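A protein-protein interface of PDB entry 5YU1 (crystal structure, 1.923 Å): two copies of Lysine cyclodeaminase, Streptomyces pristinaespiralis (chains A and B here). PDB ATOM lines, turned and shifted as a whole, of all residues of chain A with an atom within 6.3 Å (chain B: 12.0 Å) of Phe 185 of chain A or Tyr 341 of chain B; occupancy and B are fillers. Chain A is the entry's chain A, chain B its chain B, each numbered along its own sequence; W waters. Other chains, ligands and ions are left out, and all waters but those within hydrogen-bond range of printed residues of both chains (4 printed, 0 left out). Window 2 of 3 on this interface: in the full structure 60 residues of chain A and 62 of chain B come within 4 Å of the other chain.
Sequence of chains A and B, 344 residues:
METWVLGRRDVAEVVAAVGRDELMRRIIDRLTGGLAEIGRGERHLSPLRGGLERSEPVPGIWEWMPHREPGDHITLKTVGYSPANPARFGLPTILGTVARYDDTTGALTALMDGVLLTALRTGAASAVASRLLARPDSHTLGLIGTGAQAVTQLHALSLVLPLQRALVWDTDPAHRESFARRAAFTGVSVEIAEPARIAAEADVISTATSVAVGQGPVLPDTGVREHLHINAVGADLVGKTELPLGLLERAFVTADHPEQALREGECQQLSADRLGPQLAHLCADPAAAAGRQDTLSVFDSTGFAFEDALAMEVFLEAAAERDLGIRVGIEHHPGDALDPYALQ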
ATOM      1  N   VAL A  15     -10.718   0.521  10.583  1.00  0.00           N
ATOM      2  CA  VAL A  15     -11.729   0.970  11.543  1.00  0.00           C
ATOM      3  C   VAL A  15     -11.484   0.355  12.913  1.00  0.00           C
ATOM      4  O   VAL A  15     -11.618   1.026  13.944  1.00  0.00           O
ATOM      5  CB  VAL A  15     -13.142   0.635  11.037  1.00  0.00           C
ATOM      6  CG1 VAL A  15     -14.195   1.312  11.931  1.00  0.00           C
ATOM      7  CG2 VAL A  15     -13.263   1.097   9.632  1.00  0.00           C
ATOM      8  N   ARG A  20     -14.201   3.646  15.729  1.00  0.00           N
ATOM      9  CA  ARG A  20     -15.262   4.326  14.984  1.00  0.00           C
ATOM     10  C   ARG A  20     -15.277   5.824  15.261  1.00  0.00           C
ATOM     11  O   ARG A  20     -15.402   6.630  14.329  1.00  0.00           O
ATOM     12  CB  ARG A  20     -16.626   3.721  15.312  1.00  0.00           C
ATOM     13  CG  ARG A  20     -16.783   2.257  14.895  1.00  0.00           C
ATOM     14  CD  ARG A  20     -18.147   1.738  15.314  1.00  0.00           C
ATOM     15  NE  ARG A  20     -18.267   0.289  15.162  1.00  0.00           N
ATOM     16  CZ  ARG A  20     -19.224  -0.446  15.717  1.00  0.00           C
ATOM     17  NH1 ARG A  20     -20.160   0.132  16.464  1.00  0.00           N
ATOM     18  NH2 ARG A  20     -19.235  -1.762  15.537  1.00  0.00           N
ATOM     19  N   ASP A  21     -15.166   6.222  16.533  1.00  0.00           N
ATOM     20  CA  ASP A  21     -15.267   7.641  16.869  1.00  0.00           C
ATOM     21  C   ASP A  21     -14.139   8.435  16.226  1.00  0.00           C
ATOM     22  O   ASP A  21     -14.369   9.476  15.593  1.00  0.00           O
ATOM     23  CB  ASP A  21     -15.229   7.839  18.385  1.00  0.00           C
ATOM     24  CG  ASP A  21     -16.518   7.424  19.071  1.00  0.00           C
ATOM     25  OD1 ASP A  21     -17.493   7.019  18.386  1.00  0.00           O
ATOM     26  OD2 ASP A  21     -16.538   7.498  20.317  1.00  0.00           O
ATOM     27  N   MET A  24     -14.485   8.604  12.326  1.00  0.00           N
ATOM     28  CA  MET A  24     -15.518   9.563  11.941  1.00  0.00           C
ATOM     29  C   MET A  24     -15.047  10.999  12.166  1.00  0.00           C
ATOM     30  O   MET A  24     -15.275  11.869  11.322  1.00  0.00           O
ATOM     31  CB  MET A  24     -16.809   9.270  12.714  1.00  0.00           C
ATOM     32  CG  MET A  24     -17.982  10.211  12.380  1.00  0.00           C
ATOM     33  SD  MET A  24     -18.514  10.063  10.660  1.00  0.00           S
ATOM     34  CE  MET A  24     -19.687   8.721  10.748  1.00  0.00           C
ATOM     35  N   LEU A 116     -18.712   0.981   3.603  1.00  0.00           N
ATOM     36  CA  LEU A 116     -18.437   1.672   4.862  1.00  0.00           C
ATOM     37  C   LEU A 116     -18.067   3.134   4.623  1.00  0.00           C
ATOM     38  O   LEU A 116     -18.561   4.035   5.313  1.00  0.00           O
ATOM     39  CB  LEU A 116     -17.324   0.953   5.618  1.00  0.00           C
ATOM     40  CG  LEU A 116     -16.916   1.615   6.931  1.00  0.00           C
ATOM     41  CD1 LEU A 116     -18.089   1.682   7.905  1.00  0.00           C
ATOM     42  CD2 LEU A 116     -15.794   0.816   7.512  1.00  0.00           C
ATOM     43  N   LEU A 120     -19.815   6.468   6.236  1.00  0.00           N
ATOM     44  CA  LEU A 120     -19.018   7.371   7.062  1.00  0.00           C
ATOM     45  C   LEU A 120     -19.083   8.810   6.541  1.00  0.00           C
ATOM     46  O   LEU A 120     -19.323   9.751   7.309  1.00  0.00           O
ATOM     47  CB  LEU A 120     -17.559   6.890   7.121  1.00  0.00           C
ATOM     48  CG  LEU A 120     -17.283   5.586   7.890  1.00  0.00           C
ATOM     49  CD1 LEU A 120     -15.804   5.169   7.795  1.00  0.00           C
ATOM     50  CD2 LEU A 120     -17.698   5.738   9.348  1.00  0.00           C
ATOM     51  N   VAL A 151     -27.681   4.821  10.947  1.00  0.00           N
ATOM     52  CA  VAL A 151     -26.669   4.464  11.936  1.00  0.00           C
ATOM     53  C   VAL A 151     -25.559   5.500  11.973  1.00  0.00           C
ATOM     54  O   VAL A 151     -25.167   5.974  13.047  1.00  0.00           O
ATOM     55  CB  VAL A 151     -26.106   3.061  11.648  1.00  0.00           C
ATOM     56  CG1 VAL A 151     -24.907   2.771  12.595  1.00  0.00           C
ATOM     57  CG2 VAL A 151     -27.211   2.033  11.755  1.00  0.00           C
ATOM     58  N   THR A 152     -25.009   5.853  10.808  1.00  0.00           N
ATOM     59  CA  THR A 152     -23.936   6.832  10.838  1.00  0.00           C
ATOM     60  C   THR A 152     -24.446   8.257  10.940  1.00  0.00           C
ATOM     61  O   THR A 152     -23.668   9.135  11.314  1.00  0.00           O
ATOM     62  CB  THR A 152     -23.015   6.712   9.614  1.00  0.00           C
ATOM     63  OG1 THR A 152     -23.791   6.749   8.414  1.00  0.00           O
ATOM     64  CG2 THR A 152     -22.204   5.406   9.664  1.00  0.00           C
ATOM     65  N   HIS A 155     -24.458   8.393  14.709  1.00  0.00           N
ATOM     66  CA  HIS A 155     -23.084   8.391  15.199  1.00  0.00           C
ATOM     67  C   HIS A 155     -22.409   9.744  14.980  1.00  0.00           C
ATOM     68  O   HIS A 155     -21.902  10.358  15.927  1.00  0.00           O
ATOM     69  CB  HIS A 155     -22.285   7.260  14.522  1.00  0.00           C
ATOM     70  CG  HIS A 155     -20.882   7.140  15.025  1.00  0.00           C
ATOM     71  ND1 HIS A 155     -19.836   6.699  14.236  1.00  0.00           N
ATOM     72  CD2 HIS A 155     -20.349   7.426  16.237  1.00  0.00           C
ATOM     73  CE1 HIS A 155     -18.724   6.707  14.948  1.00  0.00           C
ATOM     74  NE2 HIS A 155     -19.006   7.153  16.160  1.00  0.00           N
ATOM     75  N   ALA A 156     -22.394  10.230  13.732  1.00  0.00           N
ATOM     76  CA  ALA A 156     -21.700  11.477  13.430  1.00  0.00           C
ATOM     77  C   ALA A 156     -22.280  12.650  14.206  1.00  0.00           C
ATOM     78  O   ALA A 156     -21.531  13.492  14.718  1.00  0.00           O
ATOM     79  CB  ALA A 156     -21.763  11.775  11.934  1.00  0.00           C
ATOM     80  N   ALA A 180     -32.308   0.336  17.942  1.00  0.00           N
ATOM     81  CA  ALA A 180     -31.680   0.554  19.242  1.00  0.00           C
ATOM     82  C   ALA A 180     -30.434  -0.315  19.412  1.00  0.00           C
ATOM     83  O   ALA A 180     -29.422   0.156  19.936  1.00  0.00           O
ATOM     84  CB  ALA A 180     -32.687   0.302  20.371  1.00  0.00           C
ATOM     85  N   ARG A 181     -30.476  -1.573  18.952  1.00  0.00           N
ATOM     86  CA  ARG A 181     -29.299  -2.439  19.073  1.00  0.00           C
ATOM     87  C   ARG A 181     -28.143  -1.941  18.209  1.00  0.00           C
ATOM     88  O   ARG A 181     -26.982  -1.981  18.631  1.00  0.00           O
ATOM     89  CB  ARG A 181     -29.623  -3.890  18.689  1.00  0.00           C
ATOM     90  CG  ARG A 181     -30.686  -4.610  19.506  1.00  0.00           C
ATOM     91  CD  ARG A 181     -30.843  -6.073  19.049  1.00  0.00           C
ATOM     92  NE  ARG A 181     -31.526  -6.217  17.760  1.00  0.00           N
ATOM     93  CZ  ARG A 181     -32.830  -6.446  17.622  1.00  0.00           C
ATOM     94  NH1 ARG A 181     -33.605  -6.530  18.696  1.00  0.00           N
ATOM     95  NH2 ARG A 181     -33.366  -6.577  16.413  1.00  0.00           N
ATOM     96  N   ARG A 182     -28.438  -1.504  16.980  1.00  0.00           N
ATOM     97  CA  ARG A 182     -27.389  -1.003  16.091  1.00  0.00           C
ATOM     98  C   ARG A 182     -26.814   0.320  16.588  1.00  0.00           C
ATOM     99  O   ARG A 182     -25.658   0.640  16.295  1.00  0.00           O
ATOM    100  CB  ARG A 182     -27.946  -0.854  14.665  1.00  0.00           C
ATOM    101  CG  ARG A 182     -28.196  -2.185  13.950  1.00  0.00           C
ATOM    102  CD  ARG A 182     -28.803  -1.994  12.528  1.00  0.00           C
ATOM    103  NE  ARG A 182     -30.253  -1.802  12.576  1.00  0.00           N
ATOM    104  CZ  ARG A 182     -30.906  -0.801  11.987  1.00  0.00           C
ATOM    105  NH1 ARG A 182     -30.242   0.106  11.276  1.00  0.00           N
ATOM    106  NH2 ARG A 182     -32.230  -0.708  12.106  1.00  0.00           N
ATOM    107  N   ALA A 183     -27.596   1.097  17.338  1.00  0.00           N
ATOM    108  CA  ALA A 183     -27.178   2.396  17.853  1.00  0.00           C
ATOM    109  C   ALA A 183     -26.542   2.335  19.237  1.00  0.00           C
ATOM    110  O   ALA A 183     -26.021   3.352  19.704  1.00  0.00           O
ATOM    111  CB  ALA A 183     -28.385   3.342  17.922  1.00  0.00           C
ATOM    112  N   ALA A 184     -26.572   1.174  19.900  1.00  0.00           N
ATOM    113  CA  ALA A 184     -26.251   1.115  21.329  1.00  0.00           C
ATOM    114  C   ALA A 184     -24.880   1.697  21.639  1.00  0.00           C
ATOM    115  O   ALA A 184     -24.690   2.340  22.681  1.00  0.00           O
ATOM    116  CB  ALA A 184     -26.332  -0.332  21.822  1.00  0.00           C
ATOM    117  N   PHE A 185     -23.903   1.472  20.758  1.00  0.00           N
ATOM    118  CA  PHE A 185     -22.533   1.866  21.059  1.00  0.00           C
ATOM    119  C   PHE A 185     -22.378   3.367  21.233  1.00  0.00           C
ATOM    120  O   PHE A 185     -21.422   3.805  21.883  1.00  0.00           O
ATOM    121  CB  PHE A 185     -21.585   1.361  19.964  1.00  0.00           C
ATOM    122  CG  PHE A 185     -21.594   2.190  18.703  1.00  0.00           C
ATOM    123  CD1 PHE A 185     -22.570   1.995  17.736  1.00  0.00           C
ATOM    124  CD2 PHE A 185     -20.614   3.155  18.484  1.00  0.00           C
ATOM    125  CE1 PHE A 185     -22.574   2.756  16.559  1.00  0.00           C
ATOM    126  CE2 PHE A 185     -20.609   3.919  17.310  1.00  0.00           C
ATOM    127  CZ  PHE A 185     -21.586   3.712  16.350  1.00  0.00           C
ATOM    128  N   THR A 186     -23.287   4.167  20.664  1.00  0.00           N
ATOM    129  CA  THR A 186     -23.175   5.618  20.747  1.00  0.00           C
ATOM    130  C   THR A 186     -23.563   6.166  22.105  1.00  0.00           C
ATOM    131  O   THR A 186     -23.225   7.315  22.411  1.00  0.00           O
ATOM    132  CB  THR A 186     -24.074   6.301  19.706  1.00  0.00           C
ATOM    133  OG1 THR A 186     -25.440   6.021  20.027  1.00  0.00           O
ATOM    134  CG2 THR A 186     -23.765   5.787  18.299  1.00  0.00           C
ATOM    135  N   GLY A 187     -24.285   5.395  22.908  1.00  0.00           N
ATOM    136  CA  GLY A 187     -24.769   5.877  24.179  1.00  0.00           C
ATOM    137  C   GLY A 187     -25.996   6.762  24.102  1.00  0.00           C
ATOM    138  O   GLY A 187     -26.446   7.254  25.144  1.00  0.00           O
ATOM    139  N   VAL A 188     -26.548   6.985  22.912  1.00  0.00           N
ATOM    140  CA  VAL A 188     -27.720   7.839  22.747  1.00  0.00           C
ATOM    141  C   VAL A 188     -28.953   6.955  22.879  1.00  0.00           C
ATOM    142  O   VAL A 188     -29.094   5.963  22.159  1.00  0.00           O
ATOM    143  CB  VAL A 188     -27.696   8.566  21.392  1.00  0.00           C
ATOM    144  CG1 VAL A 188     -28.966   9.393  21.213  1.00  0.00           C
ATOM    145  CG2 VAL A 188     -26.463   9.446  21.278  1.00  0.00           C
ATOM    146  N   GLU B 331     -15.825  -5.599  -1.723  1.00  0.00           N
ATOM    147  CA  GLU B 331     -17.000  -4.946  -1.156  1.00  0.00           C
ATOM    148  C   GLU B 331     -17.283  -5.459   0.246  1.00  0.00           C
ATOM    149  O   GLU B 331     -17.163  -6.657   0.528  1.00  0.00           O
ATOM    150  CB  GLU B 331     -18.239  -5.210  -2.012  1.00  0.00           C
ATOM    151  CG  GLU B 331     -18.450  -4.272  -3.145  1.00  0.00           C
ATOM    152  CD  GLU B 331     -19.633  -4.694  -4.019  1.00  0.00           C
ATOM    153  OE1 GLU B 331     -20.272  -5.736  -3.737  1.00  0.00           O
ATOM    154  OE2 GLU B 331     -19.898  -3.984  -4.997  1.00  0.00           O
ATOM    155  N   HIS B 332     -17.710  -4.549   1.110  1.00  0.00           N
ATOM    156  CA  HIS B 332     -18.089  -4.882   2.474  1.00  0.00           C
ATOM    157  C   HIS B 332     -19.563  -5.266   2.483  1.00  0.00           C
ATOM    158  O   HIS B 332     -20.423  -4.441   2.166  1.00  0.00           O
ATOM    159  CB  HIS B 332     -17.823  -3.683   3.384  1.00  0.00           C
ATOM    160  CG  HIS B 332     -18.494  -3.756   4.720  1.00  0.00           C
ATOM    161  ND1 HIS B 332     -18.614  -4.926   5.437  1.00  0.00           N
ATOM    162  CD2 HIS B 332     -19.089  -2.793   5.466  1.00  0.00           C
ATOM    163  CE1 HIS B 332     -19.237  -4.679   6.575  1.00  0.00           C
ATOM    164  NE2 HIS B 332     -19.547  -3.395   6.612  1.00  0.00           N
ATOM    165  N   HIS B 333     -19.855  -6.519   2.833  1.00  0.00           N
ATOM    166  CA  HIS B 333     -21.228  -6.994   2.961  1.00  0.00           C
ATOM    167  C   HIS B 333     -21.463  -7.248   4.443  1.00  0.00           C
ATOM    168  O   HIS B 333     -21.125  -8.328   4.957  1.00  0.00           O
ATOM    169  CB  HIS B 333     -21.471  -8.262   2.142  1.00  0.00           C
ATOM    170  CG  HIS B 333     -21.305  -8.072   0.664  1.00  0.00           C
ATOM    171  ND1 HIS B 333     -21.155  -9.129  -0.206  1.00  0.00           N
ATOM    172  CD2 HIS B 333     -21.269  -6.949  -0.095  1.00  0.00           C
ATOM    173  CE1 HIS B 333     -21.033  -8.667  -1.440  1.00  0.00           C
ATOM    174  NE2 HIS B 333     -21.103  -7.348  -1.400  1.00  0.00           N
ATOM    175  N   PRO B 334     -22.013  -6.285   5.176  1.00  0.00           N
ATOM    176  CA  PRO B 334     -22.124  -6.445   6.632  1.00  0.00           C
ATOM    177  C   PRO B 334     -23.008  -7.626   6.991  1.00  0.00           C
ATOM    178  O   PRO B 334     -23.924  -7.993   6.251  1.00  0.00           O
ATOM    179  CB  PRO B 334     -22.740  -5.121   7.095  1.00  0.00           C
ATOM    180  CG  PRO B 334     -23.434  -4.578   5.862  1.00  0.00           C
ATOM    181  CD  PRO B 334     -22.595  -5.019   4.700  1.00  0.00           C
ATOM    182  N   GLY B 335     -22.693  -8.247   8.132  1.00  0.00           N
ATOM    183  CA  GLY B 335     -23.512  -9.350   8.606  1.00  0.00           C
ATOM    184  C   GLY B 335     -24.955  -8.947   8.811  1.00  0.00           C
ATOM    185  O   GLY B 335     -25.859  -9.778   8.732  1.00  0.00           O
ATOM    186  N   ASP B 336     -25.187  -7.666   9.045  1.00  0.00           N
ATOM    187  CA  ASP B 336     -26.504  -7.073   9.187  1.00  0.00           C
ATOM    188  C   ASP B 336     -26.588  -6.015   8.095  1.00  0.00           C
ATOM    189  O   ASP B 336     -25.826  -5.045   8.119  1.00  0.00           O
ATOM    190  CB  ASP B 336     -26.645  -6.483  10.592  1.00  0.00           C
ATOM    191  CG  ASP B 336     -27.915  -5.698  10.797  1.00  0.00           C
ATOM    192  OD1 ASP B 336     -28.717  -5.521   9.849  1.00  0.00           O
ATOM    193  OD2 ASP B 336     -28.107  -5.261  11.957  1.00  0.00           O
ATOM    194  N   ALA B 337     -27.482  -6.222   7.126  1.00  0.00           N
ATOM    195  CA  ALA B 337     -27.557  -5.330   5.970  1.00  0.00           C
ATOM    196  C   ALA B 337     -27.873  -3.889   6.361  1.00  0.00           C
ATOM    197  O   ALA B 337     -27.567  -2.971   5.587  1.00  0.00           O
ATOM    198  CB  ALA B 337     -28.598  -5.845   4.977  1.00  0.00           C
ATOM    199  N   LEU B 338     -28.449  -3.662   7.544  1.00  0.00           N
ATOM    200  CA  LEU B 338     -28.789  -2.313   7.991  1.00  0.00           C
ATOM    201  C   LEU B 338     -27.743  -1.722   8.925  1.00  0.00           C
ATOM    202  O   LEU B 338     -27.991  -0.687   9.559  1.00  0.00           O
ATOM    203  CB  LEU B 338     -30.160  -2.312   8.679  1.00  0.00           C
ATOM    204  CG  LEU B 338     -31.319  -2.922   7.886  1.00  0.00           C
ATOM    205  CD1 LEU B 338     -32.634  -2.741   8.648  1.00  0.00           C
ATOM    206  CD2 LEU B 338     -31.419  -2.352   6.467  1.00  0.00           C
ATOM    207  N   ASP B 339     -26.570  -2.334   9.016  1.00  0.00           N
ATOM    208  CA  ASP B 339     -25.547  -1.889   9.954  1.00  0.00           C
ATOM    209  C   ASP B 339     -24.207  -1.783   9.240  1.00  0.00           C
ATOM    210  O   ASP B 339     -23.462  -2.767   9.145  1.00  0.00           O
ATOM    211  CB  ASP B 339     -25.469  -2.841  11.147  1.00  0.00           C
ATOM    212  CG  ASP B 339     -24.573  -2.315  12.252  1.00  0.00           C
ATOM    213  OD1 ASP B 339     -24.000  -1.209  12.098  1.00  0.00           O
ATOM    214  OD2 ASP B 339     -24.441  -3.021  13.272  1.00  0.00           O
ATOM    215  N   PRO B 340     -23.848  -0.590   8.758  1.00  0.00           N
ATOM    216  CA  PRO B 340     -22.577  -0.448   8.030  1.00  0.00           C
ATOM    217  C   PRO B 340     -21.362  -0.794   8.866  1.00  0.00           C
ATOM    218  O   PRO B 340     -20.316  -1.118   8.294  1.00  0.00           O
ATOM    219  CB  PRO B 340     -22.555   1.035   7.617  1.00  0.00           C
ATOM    220  CG  PRO B 340     -23.883   1.614   8.034  1.00  0.00           C
ATOM    221  CD  PRO B 340     -24.468   0.710   9.072  1.00  0.00           C
ATOM    222  N   TYR B 341     -21.468  -0.742  10.198  1.00  0.00           N
ATOM    223  CA  TYR B 341     -20.363  -1.090  11.086  1.00  0.00           C
ATOM    224  C   TYR B 341     -20.262  -2.587  11.373  1.00  0.00           C
ATOM    225  O   TYR B 341     -19.322  -3.004  12.058  1.00  0.00           O
ATOM    226  CB  TYR B 341     -20.497  -0.339  12.417  1.00  0.00           C
ATOM    227  CG  TYR B 341     -20.178   1.135  12.335  1.00  0.00           C
ATOM    228  CD1 TYR B 341     -18.955   1.569  11.846  1.00  0.00           C
ATOM    229  CD2 TYR B 341     -21.099   2.092  12.752  1.00  0.00           C
ATOM    230  CE1 TYR B 341     -18.638   2.904  11.776  1.00  0.00           C
ATOM    231  CE2 TYR B 341     -20.795   3.449  12.675  1.00  0.00           C
ATOM    232  CZ  TYR B 341     -19.560   3.843  12.190  1.00  0.00           C
ATOM    233  OH  TYR B 341     -19.212   5.177  12.120  1.00  0.00           O
ATOM    234  N   ALA B 342     -21.200  -3.405  10.890  1.00  0.00           N
ATOM    235  CA  ALA B 342     -21.176  -4.840  11.165  1.00  0.00           C
ATOM    236  C   ALA B 342     -20.180  -5.516  10.219  1.00  0.00           C
ATOM    237  O   ALA B 342     -20.526  -6.254   9.297  1.00  0.00           O
ATOM    238  CB  ALA B 342     -22.575  -5.432  11.048  1.00  0.00           C
ATOM    239  N   LEU B 343     -18.906  -5.255  10.466  1.00  0.00           N
ATOM    240  CA  LEU B 343     -17.871  -5.788   9.590  1.00  0.00           C
ATOM    241  C   LEU B 343     -17.739  -7.298   9.799  1.00  0.00           C
ATOM    242  O   LEU B 343     -17.711  -7.775  10.937  1.00  0.00           O
ATOM    243  CB  LEU B 343     -16.553  -5.051   9.832  1.00  0.00           C
ATOM    244  CG  LEU B 343     -16.657  -3.574   9.403  1.00  0.00           C
ATOM    245  CD1 LEU B 343     -16.101  -2.612  10.448  1.00  0.00           C
ATOM    246  CD2 LEU B 343     -16.003  -3.324   8.048  1.00  0.00           C
ATOM    247  N   GLN B 344     -17.700  -8.039   8.688  1.00  0.00           N
ATOM    248  CA  GLN B 344     -17.842  -9.506   8.649  1.00  0.00           C
ATOM    249  C   GLN B 344     -17.085 -10.251   9.748  1.00  0.00           C
ATOM    250  O   GLN B 344     -17.484 -11.338  10.174  1.00  0.00           O
ATOM    251  CB  GLN B 344     -17.386 -10.027   7.279  1.00  0.00           C
ATOM    252  CG  GLN B 344     -17.284 -11.546   7.164  1.00  0.00           C
ATOM    253  CD  GLN B 344     -16.509 -11.993   5.936  1.00  0.00           C
ATOM    254  OE1 GLN B 344     -16.736 -11.496   4.831  1.00  0.00           O
ATOM    255  NE2 GLN B 344     -15.592 -12.940   6.122  1.00  0.00           N
HETATM  256  O   HOH W   1     -30.431  -4.843  12.862  1.00  0.00           O
HETATM  257  O   HOH W   2     -21.982  -3.609  14.580  1.00  0.00           O
HETATM  258  O   HOH W   3     -16.708  -1.355  13.401  1.00  0.00           O
HETATM  259  O   HOH W   4     -23.575  -0.180  14.680  1.00  0.00           O
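ND1 of His 155 of chain A sits at hydrogen-bond distance from OH of Tyr 341 of chain B (2.7 Å). The guanidinium group of Arg 182 of chain A sits at hydrogen-bond distance from the backbone carbonyl oxygen of Leu 338 of chain B (2.9 Å).
The side-chain carboxylate (OD1) of Asp 21 of chain A sits at hydrogen-bond distance from a ring nitrogen (NE2) of His 155 of chain A (2.7 Å). A ring nitrogen (NE2) of His 332 of chain B sits at hydrogen-bond distance from the backbone carbonyl oxygen (O) of Pro 340 of chain B (2.9 Å). OD1 of Asp 336 of chain B lies within hydrogen-bond range of N of Leu 338 of chain B, 3.0 Å away. OD1 of Asp 339 of chain B lies close to N of Tyr 341 of chain B (3.2 Å).
Among the printed residues, pairs that only touch across the chains: Leu 120 of chain A with Tyr 341 of chain B, Arg 182 of chain A with Asp 336 of chain B, Arg 20 of chain A with Tyr 341 of chain B, Val 151 of chain A with Leu 338 of chain B, Leu 116 of chain A with Pro 340 of chain B, Arg 182 of chain A with Asp 339 of chain B, Phe 185 of chain A with Tyr 341 of chain B, Met 24 of chain A with Tyr 341 of chain B, Val 151 of chain A with Pro 340 of chain B, Thr 152 of chain A with Tyr 341 of chain B and Val 151 of chain A with Tyr 341 of chain B.
Of chain A, only Arg 20, Met 24, Leu 120, Val 151, Thr 152, His 155 and Phe 185 come within 4 Å of Tyr 341 of chain B. Of chain B, only Tyr 341 (3.5 Å) comes within 4 Å of Arg 20 of chain A. No residue of chain B comes within 4 Å of Asp 21 of chain A. Leu 116 of chain A touches just one residue of chain B: Pro 340 (3.6 Å). Of chain B, only Tyr 341 (3.2 Å) comes within 4 Å of Leu 120 of chain A. Thr 152 of chain A touches one residue of chain B. Of chain B, only Tyr 341 (2.7 Å) comes within 4 Å of His 155 of chain A. No residue of chain B comes within 4 Å of Ala 184 of chain A. Gly 187 of chain A touches none of the printed residues of chain B. Of the printed residues of chain A, Pro 340 of chain B touches Leu 116 (3.6 Å) and Val 151 (3.9 Å). Of the printed residues of chain A, Leu 338 of chain B touches Val 151 (3.6 Å) and Arg 182 (2.9 Å). His 332 of chain B touches none of the printed residues of chain A. Val 188 of chain A touches none of the printed residues of chain B. The nearest residue of chain B that does not touch Phe 185 of chain A is Asp 339 of chain B (6.1 Å). The nearest residue of chain A that does not touch Tyr 341 of chain B is Leu 116 of chain A (4.04 Å). The nearest printed residue of chain A that does not touch Pro 340 of chain B is Thr 152 of chain A (4.5 Å).
Of the 19 printed residues of chain A, 9 touch a printed residue of chain B. Hydrophobic or aromatic side chains of chain A that line the printed part of chain B: Met 24, Leu 116, Leu 120, Val 151, His 155 and Phe 185. Of the 14 printed residues of chain B, 5 touch a printed residue of chain A. Hydrophobic or aromatic side chains of chain B within 4 Å of the printed part of chain A: Leu 338, Pro 340 and Tyr 341. Among the printed residues, no Asp or Glu carboxylate lies within 4 Å of a Lys or Arg side-chain nitrogen of the other chain.
No position is printed for both chains.
Water W1 bridges the side-chain carboxylate of Asp 336 of chain B and the guanidinium group of Arg 182 of chain A. Water W4 bridges O of Arg 182 of chain A (2.8 Å) and OD1 of Asp 339 of chain B (2.8 Å). Water W2 bridges the side-chain carboxylate (OD2) of Asp 339 of chain B and the guanidinium group (NH2) of Arg 20 of chain A. Water W3 bridges the guanidinium group (NE) of Arg 20 of chain A (2.9 Å) and the backbone carbonyl oxygen (O) of Tyr 341 of chain B (3.4 Å).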
